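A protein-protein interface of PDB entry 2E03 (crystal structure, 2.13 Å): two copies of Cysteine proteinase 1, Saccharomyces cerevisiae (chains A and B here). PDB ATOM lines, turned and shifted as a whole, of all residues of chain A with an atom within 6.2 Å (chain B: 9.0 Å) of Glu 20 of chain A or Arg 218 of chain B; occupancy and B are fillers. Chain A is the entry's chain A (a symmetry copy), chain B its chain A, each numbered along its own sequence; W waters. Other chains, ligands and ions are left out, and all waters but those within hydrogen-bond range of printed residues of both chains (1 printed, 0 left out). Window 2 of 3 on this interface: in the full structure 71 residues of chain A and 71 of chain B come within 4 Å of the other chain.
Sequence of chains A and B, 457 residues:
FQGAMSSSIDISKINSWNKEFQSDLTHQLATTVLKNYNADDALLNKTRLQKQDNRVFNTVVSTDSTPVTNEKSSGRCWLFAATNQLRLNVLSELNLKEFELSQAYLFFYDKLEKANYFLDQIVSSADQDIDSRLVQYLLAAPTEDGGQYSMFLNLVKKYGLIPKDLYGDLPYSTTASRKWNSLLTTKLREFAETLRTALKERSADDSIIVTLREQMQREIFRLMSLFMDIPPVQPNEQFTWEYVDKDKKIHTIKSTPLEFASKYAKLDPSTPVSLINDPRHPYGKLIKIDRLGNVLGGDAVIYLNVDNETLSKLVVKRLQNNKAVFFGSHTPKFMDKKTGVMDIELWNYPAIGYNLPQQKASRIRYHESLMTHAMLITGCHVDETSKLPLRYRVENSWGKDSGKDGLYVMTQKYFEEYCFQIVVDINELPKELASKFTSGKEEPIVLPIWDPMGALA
Of the 10 printed residues of chain A, 4 touch a printed residue of chain B.
Hydrophobic or aromatic side chains of chain A that line the printed part of chain B: Trp 17 and Phe 21.
Of the 19 printed residues of chain B, 5 touch a printed residue of chain A.
Hydrophobic or aromatic side chains of chain B that line the printed part of chain A: Phe 221.
Along chain B the printed residues that touch a printed residue of chain A span positions 214 to 222.
Water W1 lies within hydrogen-bond range of the backbone carbonyl oxygen (O) of Ser 225 of chain B (2.5 Å) and the side-chain amide nitrogen (NE2) of Gln 22 of chain A (3.2 Å).
Among the printed residues, merely in contact across the chains: Trp 17 of chain A with Glu 214 of chain B (3.8 Å), Trp 17 of chain A with Gln 217 of chain B (3.8 Å), Trp 17 of chain A with Arg 218 of chain B (3.5 Å), Asn 18 of chain A with Phe 221 of chain B (3.7 Å), Phe 21 of chain A with Arg 218 of chain B (3.6 Å), Phe 21 of chain A with Phe 221 of chain B (3.9 Å) and Phe 21 of chain A with Arg 222 of chain B (3.5 Å).
The side-chain carboxylate (OE2) of Glu 20 of chain A lies within salt-bridge range of the guanidinium group (NH2) of Arg 218 of chain B (2.7 Å).
Of chain A, only Trp 17 (3.5 Å), Glu 20 (2.7 Å) and Phe 21 (3.6 Å) come within 4 Å of Arg 218 of chain B.
Trp 17 of chain A touches just these residues of chain B: Glu 214 (3.8 Å), Gln 217 (3.8 Å) and Arg 218 (3.5 Å).
Of the printed residues of chain A, Arg 222 of chain B touches Phe 21 (3.5 Å).
Printed residues of chain B within 4 Å of Phe 21 of chain A: Arg 218, Phe 221 and Arg 222.
Of the printed residues of chain B, Asn 18 of chain A touches Phe 221 (3.7 Å).
The nearest residue of chain B that does not touch Glu 20 of chain A is Phe 221 of chain B (7.7 Å).
The nearest printed residue of chain A that does not touch Arg 218 of chain B is Ser 16 of chain A (7.5 Å).
No position is printed for both chains.
Of the 8 pairs that touch across the chains among the printed residues, none has its exchanged pair printed and touching as well.
The side-chain amide nitrogen (NE2) of Gln 217 of chain B sits at hydrogen-bond distance from the side-chain amide oxygen (OD1) of Asn 116 of chain B, at 2.7 Å.
OE2 of Glu 219 of chain B is in salt-bridge range of NH1 of Arg 222 of chain B (2.7 Å).
The side-chain hydroxyl (OG) of Ser 225 of chain B lies within hydrogen-bond range of the backbone carbonyl oxygen (O) of Arg 222 of chain B, 2.7 Å away.
The side-chain hydroxyl of Ser 23 of chain A is in hydrogen-bond range of the backbone carbonyl oxygen of Glu 20 of chain A, 2.7 Å away.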
ATOM      1  N   ASN A  15      24.575  26.218 -19.257  1.00  0.00           N
ATOM      2  CA  ASN A  15      25.748  25.498 -19.701  1.00  0.00           C
ATOM      3  C   ASN A  15      26.791  25.430 -18.548  1.00  0.00           C
ATOM      4  O   ASN A  15      27.497  24.412 -18.390  1.00  0.00           O
ATOM      5  CB  ASN A  15      26.283  26.201 -20.971  1.00  0.00           C
ATOM      6  CG  ASN A  15      25.590  25.687 -22.208  1.00  0.00           C
ATOM      7  OD1 ASN A  15      25.967  24.652 -22.691  1.00  0.00           O
ATOM      8  ND2 ASN A  15      24.558  26.397 -22.711  1.00  0.00           N
ATOM      9  N   SER A  16      26.827  26.466 -17.699  1.00  0.00           N
ATOM     10  CA  SER A  16      27.761  26.456 -16.563  1.00  0.00           C
ATOM     11  C   SER A  16      27.232  25.476 -15.506  1.00  0.00           C
ATOM     12  O   SER A  16      27.986  24.687 -14.915  1.00  0.00           O
ATOM     13  CB  SER A  16      27.866  27.878 -15.976  1.00  0.00           C
ATOM     14  OG  SER A  16      28.295  28.786 -16.987  1.00  0.00           O
ATOM     15  N   TRP A  17      25.927  25.472 -15.316  1.00  0.00           N
ATOM     16  CA  TRP A  17      25.333  24.542 -14.368  1.00  0.00           C
ATOM     17  C   TRP A  17      25.584  23.114 -14.911  1.00  0.00           C
ATOM     18  O   TRP A  17      25.908  22.171 -14.171  1.00  0.00           O
ATOM     19  CB  TRP A  17      23.825  24.800 -14.265  1.00  0.00           C
ATOM     20  CG  TRP A  17      23.457  26.014 -13.545  1.00  0.00           C
ATOM     21  CD1 TRP A  17      24.227  26.702 -12.595  1.00  0.00           C
ATOM     22  CD2 TRP A  17      22.211  26.738 -13.647  1.00  0.00           C
ATOM     23  NE1 TRP A  17      23.525  27.791 -12.140  1.00  0.00           N
ATOM     24  CE2 TRP A  17      22.293  27.839 -12.756  1.00  0.00           C
ATOM     25  CE3 TRP A  17      21.037  26.551 -14.392  1.00  0.00           C
ATOM     26  CZ2 TRP A  17      21.232  28.767 -12.593  1.00  0.00           C
ATOM     27  CZ3 TRP A  17      19.972  27.469 -14.234  1.00  0.00           C
ATOM     28  CH2 TRP A  17      20.085  28.568 -13.339  1.00  0.00           C
ATOM     29  N   ASN A  18      25.384  22.947 -16.203  1.00  0.00           N
ATOM     30  CA  ASN A  18      25.607  21.641 -16.807  1.00  0.00           C
ATOM     31  C   ASN A  18      27.056  21.186 -16.511  1.00  0.00           C
ATOM     32  O   ASN A  18      27.270  20.033 -16.149  1.00  0.00           O
ATOM     33  CB  ASN A  18      25.456  21.661 -18.335  1.00  0.00           C
ATOM     34  CG  ASN A  18      25.536  20.231 -18.918  1.00  0.00           C
ATOM     35  OD1 ASN A  18      24.815  19.354 -18.475  1.00  0.00           O
ATOM     36  ND2 ASN A  18      26.447  19.994 -19.842  1.00  0.00           N
ATOM     37  N   LYS A  19      28.043  22.078 -16.692  1.00  0.00           N
ATOM     38  CA  LYS A  19      29.451  21.714 -16.405  1.00  0.00           C
ATOM     39  C   LYS A  19      29.587  21.272 -14.921  1.00  0.00           C
ATOM     40  O   LYS A  19      30.250  20.265 -14.608  1.00  0.00           O
ATOM     41  CB  LYS A  19      30.383  22.891 -16.712  1.00  0.00           C
ATOM     42  CG  LYS A  19      31.840  22.671 -16.395  1.00  0.00           C
ATOM     43  CD  LYS A  19      32.667  23.774 -17.082  1.00  0.00           C
ATOM     44  CE  LYS A  19      34.026  24.047 -16.423  1.00  0.00           C
ATOM     45  NZ  LYS A  19      34.949  22.999 -16.784  1.00  0.00           N
ATOM     46  N   GLU A  20      28.969  22.005 -14.009  1.00  0.00           N
ATOM     47  CA  GLU A  20      29.024  21.649 -12.606  1.00  0.00           C
ATOM     48  C   GLU A  20      28.370  20.250 -12.353  1.00  0.00           C
ATOM     49  O   GLU A  20      28.954  19.358 -11.729  1.00  0.00           O
ATOM     50  CB  GLU A  20      28.311  22.711 -11.785  1.00  0.00           C
ATOM     51  CG  GLU A  20      28.312  22.283 -10.331  1.00  0.00           C
ATOM     52  CD  GLU A  20      27.806  23.332  -9.399  1.00  0.00           C
ATOM     53  OE1 GLU A  20      27.993  24.539  -9.664  1.00  0.00           O
ATOM     54  OE2 GLU A  20      27.225  22.964  -8.372  1.00  0.00           O
ATOM     55  N   PHE A  21      27.155  20.053 -12.840  1.00  0.00           N
ATOM     56  CA  PHE A  21      26.527  18.765 -12.632  1.00  0.00           C
ATOM     57  C   PHE A  21      27.339  17.601 -13.237  1.00  0.00           C
ATOM     58  O   PHE A  21      27.435  16.572 -12.636  1.00  0.00           O
ATOM     59  CB  PHE A  21      25.093  18.750 -13.196  1.00  0.00           C
ATOM     60  CG  PHE A  21      24.197  19.800 -12.615  1.00  0.00           C
ATOM     61  CD1 PHE A  21      24.286  20.157 -11.302  1.00  0.00           C
ATOM     62  CD2 PHE A  21      23.250  20.440 -13.406  1.00  0.00           C
ATOM     63  CE1 PHE A  21      23.453  21.140 -10.784  1.00  0.00           C
ATOM     64  CE2 PHE A  21      22.440  21.398 -12.887  1.00  0.00           C
ATOM     65  CZ  PHE A  21      22.540  21.750 -11.584  1.00  0.00           C
ATOM     66  N   GLN A  22      27.953  17.778 -14.405  1.00  0.00           N
ATOM     67  CA  GLN A  22      28.693  16.687 -15.001  1.00  0.00           C
ATOM     68  C   GLN A  22      30.020  16.391 -14.246  1.00  0.00           C
ATOM     69  O   GLN A  22      30.619  15.368 -14.480  1.00  0.00           O
ATOM     70  CB  GLN A  22      28.987  16.955 -16.478  1.00  0.00           C
ATOM     71  CG  GLN A  22      27.774  17.049 -17.405  1.00  0.00           C
ATOM     72  CD  GLN A  22      26.956  15.747 -17.563  1.00  0.00           C
ATOM     73  OE1 GLN A  22      27.520  14.640 -17.648  1.00  0.00           O
ATOM     74  NE2 GLN A  22      25.605  15.896 -17.638  1.00  0.00           N
ATOM     75  N   SER A  23      30.457  17.263 -13.344  1.00  0.00           N
ATOM     76  CA  SER A  23      31.663  16.974 -12.544  1.00  0.00           C
ATOM     77  C   SER A  23      31.295  16.041 -11.371  1.00  0.00           C
ATOM     78  O   SER A  23      32.178  15.509 -10.727  1.00  0.00           O
ATOM     79  CB  SER A  23      32.302  18.285 -11.984  1.00  0.00           C
ATOM     80  OG  SER A  23      31.523  18.851 -10.935  1.00  0.00           O
ATOM     81  N   ASP A  24      29.997  15.845 -11.101  1.00  0.00           N
ATOM     82  CA  ASP A  24      29.557  14.964  -9.999  1.00  0.00           C
ATOM     83  C   ASP A  24      29.343  13.543 -10.543  1.00  0.00           C
ATOM     84  O   ASP A  24      28.623  13.330 -11.545  1.00  0.00           O
ATOM     85  CB  ASP A  24      28.231  15.464  -9.411  1.00  0.00           C
ATOM     86  CG  ASP A  24      27.720  14.578  -8.274  1.00  0.00           C
ATOM     87  OD1 ASP A  24      28.270  14.641  -7.158  1.00  0.00           O
ATOM     88  OD2 ASP A  24      26.782  13.804  -8.485  1.00  0.00           O
ATOM     89  N   LEU B 112      12.265  23.242 -21.312  1.00  0.00           N
ATOM     90  CA  LEU B 112      13.024  24.029 -20.328  1.00  0.00           C
ATOM     91  C   LEU B 112      12.334  25.411 -20.258  1.00  0.00           C
ATOM     92  O   LEU B 112      12.033  25.894 -19.180  1.00  0.00           O
ATOM     93  CB  LEU B 112      14.471  24.230 -20.832  1.00  0.00           C
ATOM     94  CG  LEU B 112      15.619  24.411 -19.803  1.00  0.00           C
ATOM     95  CD1 LEU B 112      16.677  25.284 -20.441  1.00  0.00           C
ATOM     96  CD2 LEU B 112      15.177  24.948 -18.451  1.00  0.00           C
ATOM     97  N   ASN B 116      10.215  27.208 -17.181  1.00  0.00           N
ATOM     98  CA  ASN B 116      10.616  28.527 -16.694  1.00  0.00           C
ATOM     99  C   ASN B 116       9.442  29.527 -16.812  1.00  0.00           C
ATOM    100  O   ASN B 116       9.255  30.335 -15.927  1.00  0.00           O
ATOM    101  CB  ASN B 116      11.806  29.081 -17.496  1.00  0.00           C
ATOM    102  CG  ASN B 116      12.249  30.462 -16.998  1.00  0.00           C
ATOM    103  OD1 ASN B 116      12.767  30.590 -15.873  1.00  0.00           O
ATOM    104  ND2 ASN B 116      12.048  31.501 -17.823  1.00  0.00           N
ATOM    105  N   LEU B 119       6.925  29.318 -13.955  1.00  0.00           N
ATOM    106  CA  LEU B 119       7.319  29.978 -12.707  1.00  0.00           C
ATOM    107  C   LEU B 119       6.934  31.447 -12.779  1.00  0.00           C
ATOM    108  O   LEU B 119       6.427  31.986 -11.792  1.00  0.00           O
ATOM    109  CB  LEU B 119       8.811  29.889 -12.465  1.00  0.00           C
ATOM    110  CG  LEU B 119       9.466  28.533 -12.393  1.00  0.00           C
ATOM    111  CD1 LEU B 119      11.008  28.767 -12.339  1.00  0.00           C
ATOM    112  CD2 LEU B 119       9.001  27.789 -11.142  1.00  0.00           C
ATOM    113  N   PHE B 191       7.125  23.901  -6.363  1.00  0.00           N
ATOM    114  CA  PHE B 191       7.713  25.206  -6.572  1.00  0.00           C
ATOM    115  C   PHE B 191       6.666  26.337  -6.543  1.00  0.00           C
ATOM    116  O   PHE B 191       6.900  27.404  -5.957  1.00  0.00           O
ATOM    117  CB  PHE B 191       8.504  25.240  -7.907  1.00  0.00           C
ATOM    118  CG  PHE B 191       9.863  24.476  -7.860  1.00  0.00           C
ATOM    119  CD1 PHE B 191      10.323  23.905  -6.672  1.00  0.00           C
ATOM    120  CD2 PHE B 191      10.669  24.349  -9.013  1.00  0.00           C
ATOM    121  CE1 PHE B 191      11.560  23.207  -6.580  1.00  0.00           C
ATOM    122  CE2 PHE B 191      11.933  23.647  -8.957  1.00  0.00           C
ATOM    123  CZ  PHE B 191      12.369  23.075  -7.725  1.00  0.00           C
ATOM    124  N   THR B 211      16.415  35.094  -5.944  1.00  0.00           N
ATOM    125  CA  THR B 211      17.321  33.988  -5.641  1.00  0.00           C
ATOM    126  C   THR B 211      16.529  32.666  -5.712  1.00  0.00           C
ATOM    127  O   THR B 211      16.976  31.704  -6.308  1.00  0.00           O
ATOM    128  CB  THR B 211      17.912  34.176  -4.187  1.00  0.00           C
ATOM    129  OG1 THR B 211      18.760  35.337  -4.188  1.00  0.00           O
ATOM    130  CG2 THR B 211      18.711  32.963  -3.712  1.00  0.00           C
ATOM    131  N   LEU B 212      15.342  32.655  -5.104  1.00  0.00           N
ATOM    132  CA  LEU B 212      14.494  31.460  -5.046  1.00  0.00           C
ATOM    133  C   LEU B 212      14.216  31.016  -6.462  1.00  0.00           C
ATOM    134  O   LEU B 212      14.409  29.837  -6.829  1.00  0.00           O
ATOM    135  CB  LEU B 212      13.189  31.784  -4.290  1.00  0.00           C
ATOM    136  CG  LEU B 212      12.249  30.711  -3.723  1.00  0.00           C
ATOM    137  CD1 LEU B 212      13.023  29.615  -3.053  1.00  0.00           C
ATOM    138  CD2 LEU B 212      11.255  31.386  -2.744  1.00  0.00           C
ATOM    139  N   ARG B 213      13.836  31.973  -7.291  1.00  0.00           N
ATOM    140  CA  ARG B 213      13.516  31.644  -8.684  1.00  0.00           C
ATOM    141  C   ARG B 213      14.736  31.077  -9.435  1.00  0.00           C
ATOM    142  O   ARG B 213      14.601  30.179 -10.264  1.00  0.00           O
ATOM    143  CB  ARG B 213      12.984  32.867  -9.420  1.00  0.00           C
ATOM    144  CG  ARG B 213      11.587  33.304  -8.931  1.00  0.00           C
ATOM    145  CD  ARG B 213      11.153  34.523  -9.647  1.00  0.00           C
ATOM    146  NE  ARG B 213      10.777  34.233 -11.018  1.00  0.00           N
ATOM    147  CZ  ARG B 213      10.042  35.054 -11.769  1.00  0.00           C
ATOM    148  NH1 ARG B 213       9.620  36.225 -11.278  1.00  0.00           N
ATOM    149  NH2 ARG B 213       9.707  34.697 -12.995  1.00  0.00           N
ATOM    150  N   GLU B 214      15.930  31.566  -9.116  1.00  0.00           N
ATOM    151  CA  GLU B 214      17.105  31.059  -9.827  1.00  0.00           C
ATOM    152  C   GLU B 214      17.390  29.666  -9.422  1.00  0.00           C
ATOM    153  O   GLU B 214      17.760  28.864 -10.267  1.00  0.00           O
ATOM    154  CB  GLU B 214      18.352  31.880  -9.594  1.00  0.00           C
ATOM    155  CG  GLU B 214      19.430  31.504 -10.600  1.00  0.00           C
ATOM    156  CD  GLU B 214      20.635  32.408 -10.477  1.00  0.00           C
ATOM    157  OE1 GLU B 214      21.270  32.392  -9.414  1.00  0.00           O
ATOM    158  OE2 GLU B 214      20.941  33.130 -11.414  1.00  0.00           O
ATOM    159  N   GLN B 215      17.257  29.386  -8.131  1.00  0.00           N
ATOM    160  CA  GLN B 215      17.458  28.014  -7.666  1.00  0.00           C
ATOM    161  C   GLN B 215      16.463  27.012  -8.344  1.00  0.00           C
ATOM    162  O   GLN B 215      16.818  25.841  -8.593  1.00  0.00           O
ATOM    163  CB  GLN B 215      17.302  27.944  -6.152  1.00  0.00           C
ATOM    164  CG  GLN B 215      18.270  28.871  -5.481  1.00  0.00           C
ATOM    165  CD  GLN B 215      18.143  28.843  -3.977  1.00  0.00           C
ATOM    166  OE1 GLN B 215      17.034  28.831  -3.417  1.00  0.00           O
ATOM    167  NE2 GLN B 215      19.281  28.835  -3.305  1.00  0.00           N
ATOM    168  N   MET B 216      15.248  27.485  -8.651  1.00  0.00           N
ATOM    169  CA  MET B 216      14.237  26.653  -9.294  1.00  0.00           C
ATOM    170  C   MET B 216      14.620  26.391 -10.740  1.00  0.00           C
ATOM    171  O   MET B 216      14.461  25.262 -11.254  1.00  0.00           O
ATOM    172  CB  MET B 216      12.843  27.326  -9.187  1.00  0.00           C
ATOM    173  CG  MET B 216      12.344  27.261  -7.768  1.00  0.00           C
ATOM    174  SD  MET B 216      10.861  28.286  -7.536  1.00  0.00           S
ATOM    175  CE  MET B 216      10.510  27.775  -5.912  1.00  0.00           C
ATOM    176  N   GLN B 217      15.096  27.427 -11.426  1.00  0.00           N
ATOM    177  CA  GLN B 217      15.571  27.211 -12.766  1.00  0.00           C
ATOM    178  C   GLN B 217      16.707  26.134 -12.739  1.00  0.00           C
ATOM    179  O   GLN B 217      16.737  25.222 -13.546  1.00  0.00           O
ATOM    180  CB  GLN B 217      16.156  28.481 -13.380  1.00  0.00           C
ATOM    181  CG  GLN B 217      15.227  29.692 -13.663  1.00  0.00           C
ATOM    182  CD  GLN B 217      15.970  30.775 -14.473  1.00  0.00           C
ATOM    183  OE1 GLN B 217      17.239  30.901 -14.395  1.00  0.00           O
ATOM    184  NE2 GLN B 217      15.220  31.550 -15.243  1.00  0.00           N
ATOM    185  N   ARG B 218      17.608  26.265 -11.781  1.00  0.00           N
ATOM    186  CA  ARG B 218      18.744  25.366 -11.666  1.00  0.00           C
ATOM    187  C   ARG B 218      18.289  23.930 -11.506  1.00  0.00           C
ATOM    188  O   ARG B 218      18.806  23.023 -12.153  1.00  0.00           O
ATOM    189  CB  ARG B 218      19.605  25.754 -10.440  1.00  0.00           C
ATOM    190  CG  ARG B 218      21.031  25.149 -10.433  1.00  0.00           C
ATOM    191  CD  ARG B 218      21.866  25.861  -9.329  1.00  0.00           C
ATOM    192  NE  ARG B 218      23.187  25.254  -9.163  1.00  0.00           N
ATOM    193  CZ  ARG B 218      23.350  24.110  -8.499  1.00  0.00           C
ATOM    194  NH1 ARG B 218      22.275  23.510  -7.986  1.00  0.00           N
ATOM    195  NH2 ARG B 218      24.552  23.576  -8.318  1.00  0.00           N
ATOM    196  N   GLU B 219      17.323  23.759 -10.620  1.00  0.00           N
ATOM    197  CA  GLU B 219      16.764  22.465 -10.273  1.00  0.00           C
ATOM    198  C   GLU B 219      15.983  21.889 -11.463  1.00  0.00           C
ATOM    199  O   GLU B 219      16.090  20.713 -11.750  1.00  0.00           O
ATOM    200  CB  GLU B 219      15.893  22.646  -9.039  1.00  0.00           C
ATOM    201  CG  GLU B 219      15.593  21.402  -8.300  1.00  0.00           C
ATOM    202  CD  GLU B 219      16.831  20.613  -7.837  1.00  0.00           C
ATOM    203  OE1 GLU B 219      18.027  20.993  -8.090  1.00  0.00           O
ATOM    204  OE2 GLU B 219      16.561  19.580  -7.205  1.00  0.00           O
ATOM    205  N   ILE B 220      15.241  22.725 -12.184  1.00  0.00           N
ATOM    206  CA  ILE B 220      14.526  22.246 -13.377  1.00  0.00           C
ATOM    207  C   ILE B 220      15.568  21.712 -14.424  1.00  0.00           C
ATOM    208  O   ILE B 220      15.465  20.591 -14.949  1.00  0.00           O
ATOM    209  CB  ILE B 220      13.678  23.401 -13.988  1.00  0.00           C
ATOM    210  CG1 ILE B 220      12.509  23.723 -13.060  1.00  0.00           C
ATOM    211  CG2 ILE B 220      13.202  23.015 -15.395  1.00  0.00           C
ATOM    212  CD1 ILE B 220      11.930  25.058 -13.421  1.00  0.00           C
ATOM    213  N   PHE B 221      16.595  22.518 -14.669  1.00  0.00           N
ATOM    214  CA  PHE B 221      17.639  22.155 -15.603  1.00  0.00           C
ATOM    215  C   PHE B 221      18.383  20.859 -15.212  1.00  0.00           C
ATOM    216  O   PHE B 221      18.653  19.996 -16.071  1.00  0.00           O
ATOM    217  CB  PHE B 221      18.660  23.305 -15.746  1.00  0.00           C
ATOM    218  CG  PHE B 221      19.738  22.994 -16.719  1.00  0.00           C
ATOM    219  CD1 PHE B 221      19.441  22.895 -18.073  1.00  0.00           C
ATOM    220  CD2 PHE B 221      21.001  22.586 -16.270  1.00  0.00           C
ATOM    221  CE1 PHE B 221      20.373  22.363 -18.991  1.00  0.00           C
ATOM    222  CE2 PHE B 221      21.945  22.065 -17.186  1.00  0.00           C
ATOM    223  CZ  PHE B 221      21.618  21.950 -18.543  1.00  0.00           C
ATOM    224  N   ARG B 222      18.709  20.757 -13.932  1.00  0.00           N
ATOM    225  CA  ARG B 222      19.397  19.626 -13.366  1.00  0.00           C
ATOM    226  C   ARG B 222      18.539  18.388 -13.675  1.00  0.00           C
ATOM    227  O   ARG B 222      19.036  17.440 -14.274  1.00  0.00           O
ATOM    228  CB  ARG B 222      19.541  19.819 -11.854  1.00  0.00           C
ATOM    229  CG  ARG B 222      20.465  18.851 -11.082  1.00  0.00           C
ATOM    230  CD  ARG B 222      20.055  18.845  -9.572  1.00  0.00           C
ATOM    231  NE  ARG B 222      19.961  17.448  -9.279  1.00  0.00           N
ATOM    232  CZ  ARG B 222      18.988  16.803  -8.657  1.00  0.00           C
ATOM    233  NH1 ARG B 222      17.887  17.382  -8.156  1.00  0.00           N
ATOM    234  NH2 ARG B 222      19.153  15.518  -8.573  1.00  0.00           N
ATOM    235  N   LEU B 223      17.269  18.432 -13.280  1.00  0.00           N
ATOM    236  CA  LEU B 223      16.354  17.333 -13.527  1.00  0.00           C
ATOM    237  C   LEU B 223      16.241  17.069 -15.040  1.00  0.00           C
ATOM    238  O   LEU B 223      16.213  15.924 -15.460  1.00  0.00           O
ATOM    239  CB  LEU B 223      14.977  17.643 -12.926  1.00  0.00           C
ATOM    240  CG  LEU B 223      15.025  17.537 -11.367  1.00  0.00           C
ATOM    241  CD1 LEU B 223      13.696  17.902 -10.804  1.00  0.00           C
ATOM    242  CD2 LEU B 223      15.442  16.131 -10.878  1.00  0.00           C
ATOM    243  N   MET B 224      16.160  18.119 -15.860  1.00  0.00           N
ATOM    244  CA  MET B 224      16.052  17.873 -17.289  1.00  0.00           C
ATOM    245  C   MET B 224      17.260  17.153 -17.876  1.00  0.00           C
ATOM    246  O   MET B 224      17.112  16.301 -18.754  1.00  0.00           O
ATOM    247  CB  MET B 224      15.875  19.174 -18.041  1.00  0.00           C
ATOM    248  CG  MET B 224      14.426  19.643 -17.890  1.00  0.00           C
ATOM    249  SD  MET B 224      13.946  20.863 -19.036  1.00  0.00           S
ATOM    250  CE  MET B 224      14.146  20.011 -20.607  1.00  0.00           C
ATOM    251  N   SER B 225      18.449  17.487 -17.350  1.00  0.00           N
ATOM    252  CA  SER B 225      19.678  16.955 -17.874  1.00  0.00           C
ATOM    253  C   SER B 225      19.877  15.512 -17.546  1.00  0.00           C
ATOM    254  O   SER B 225      20.783  14.901 -18.100  1.00  0.00           O
ATOM    255  CB  SER B 225      20.878  17.777 -17.396  1.00  0.00           C
ATOM    256  OG  SER B 225      21.102  17.470 -16.069  1.00  0.00           O
HETATM  257  O   HOH W   1      22.873  15.429 -19.304  1.00  0.00           O
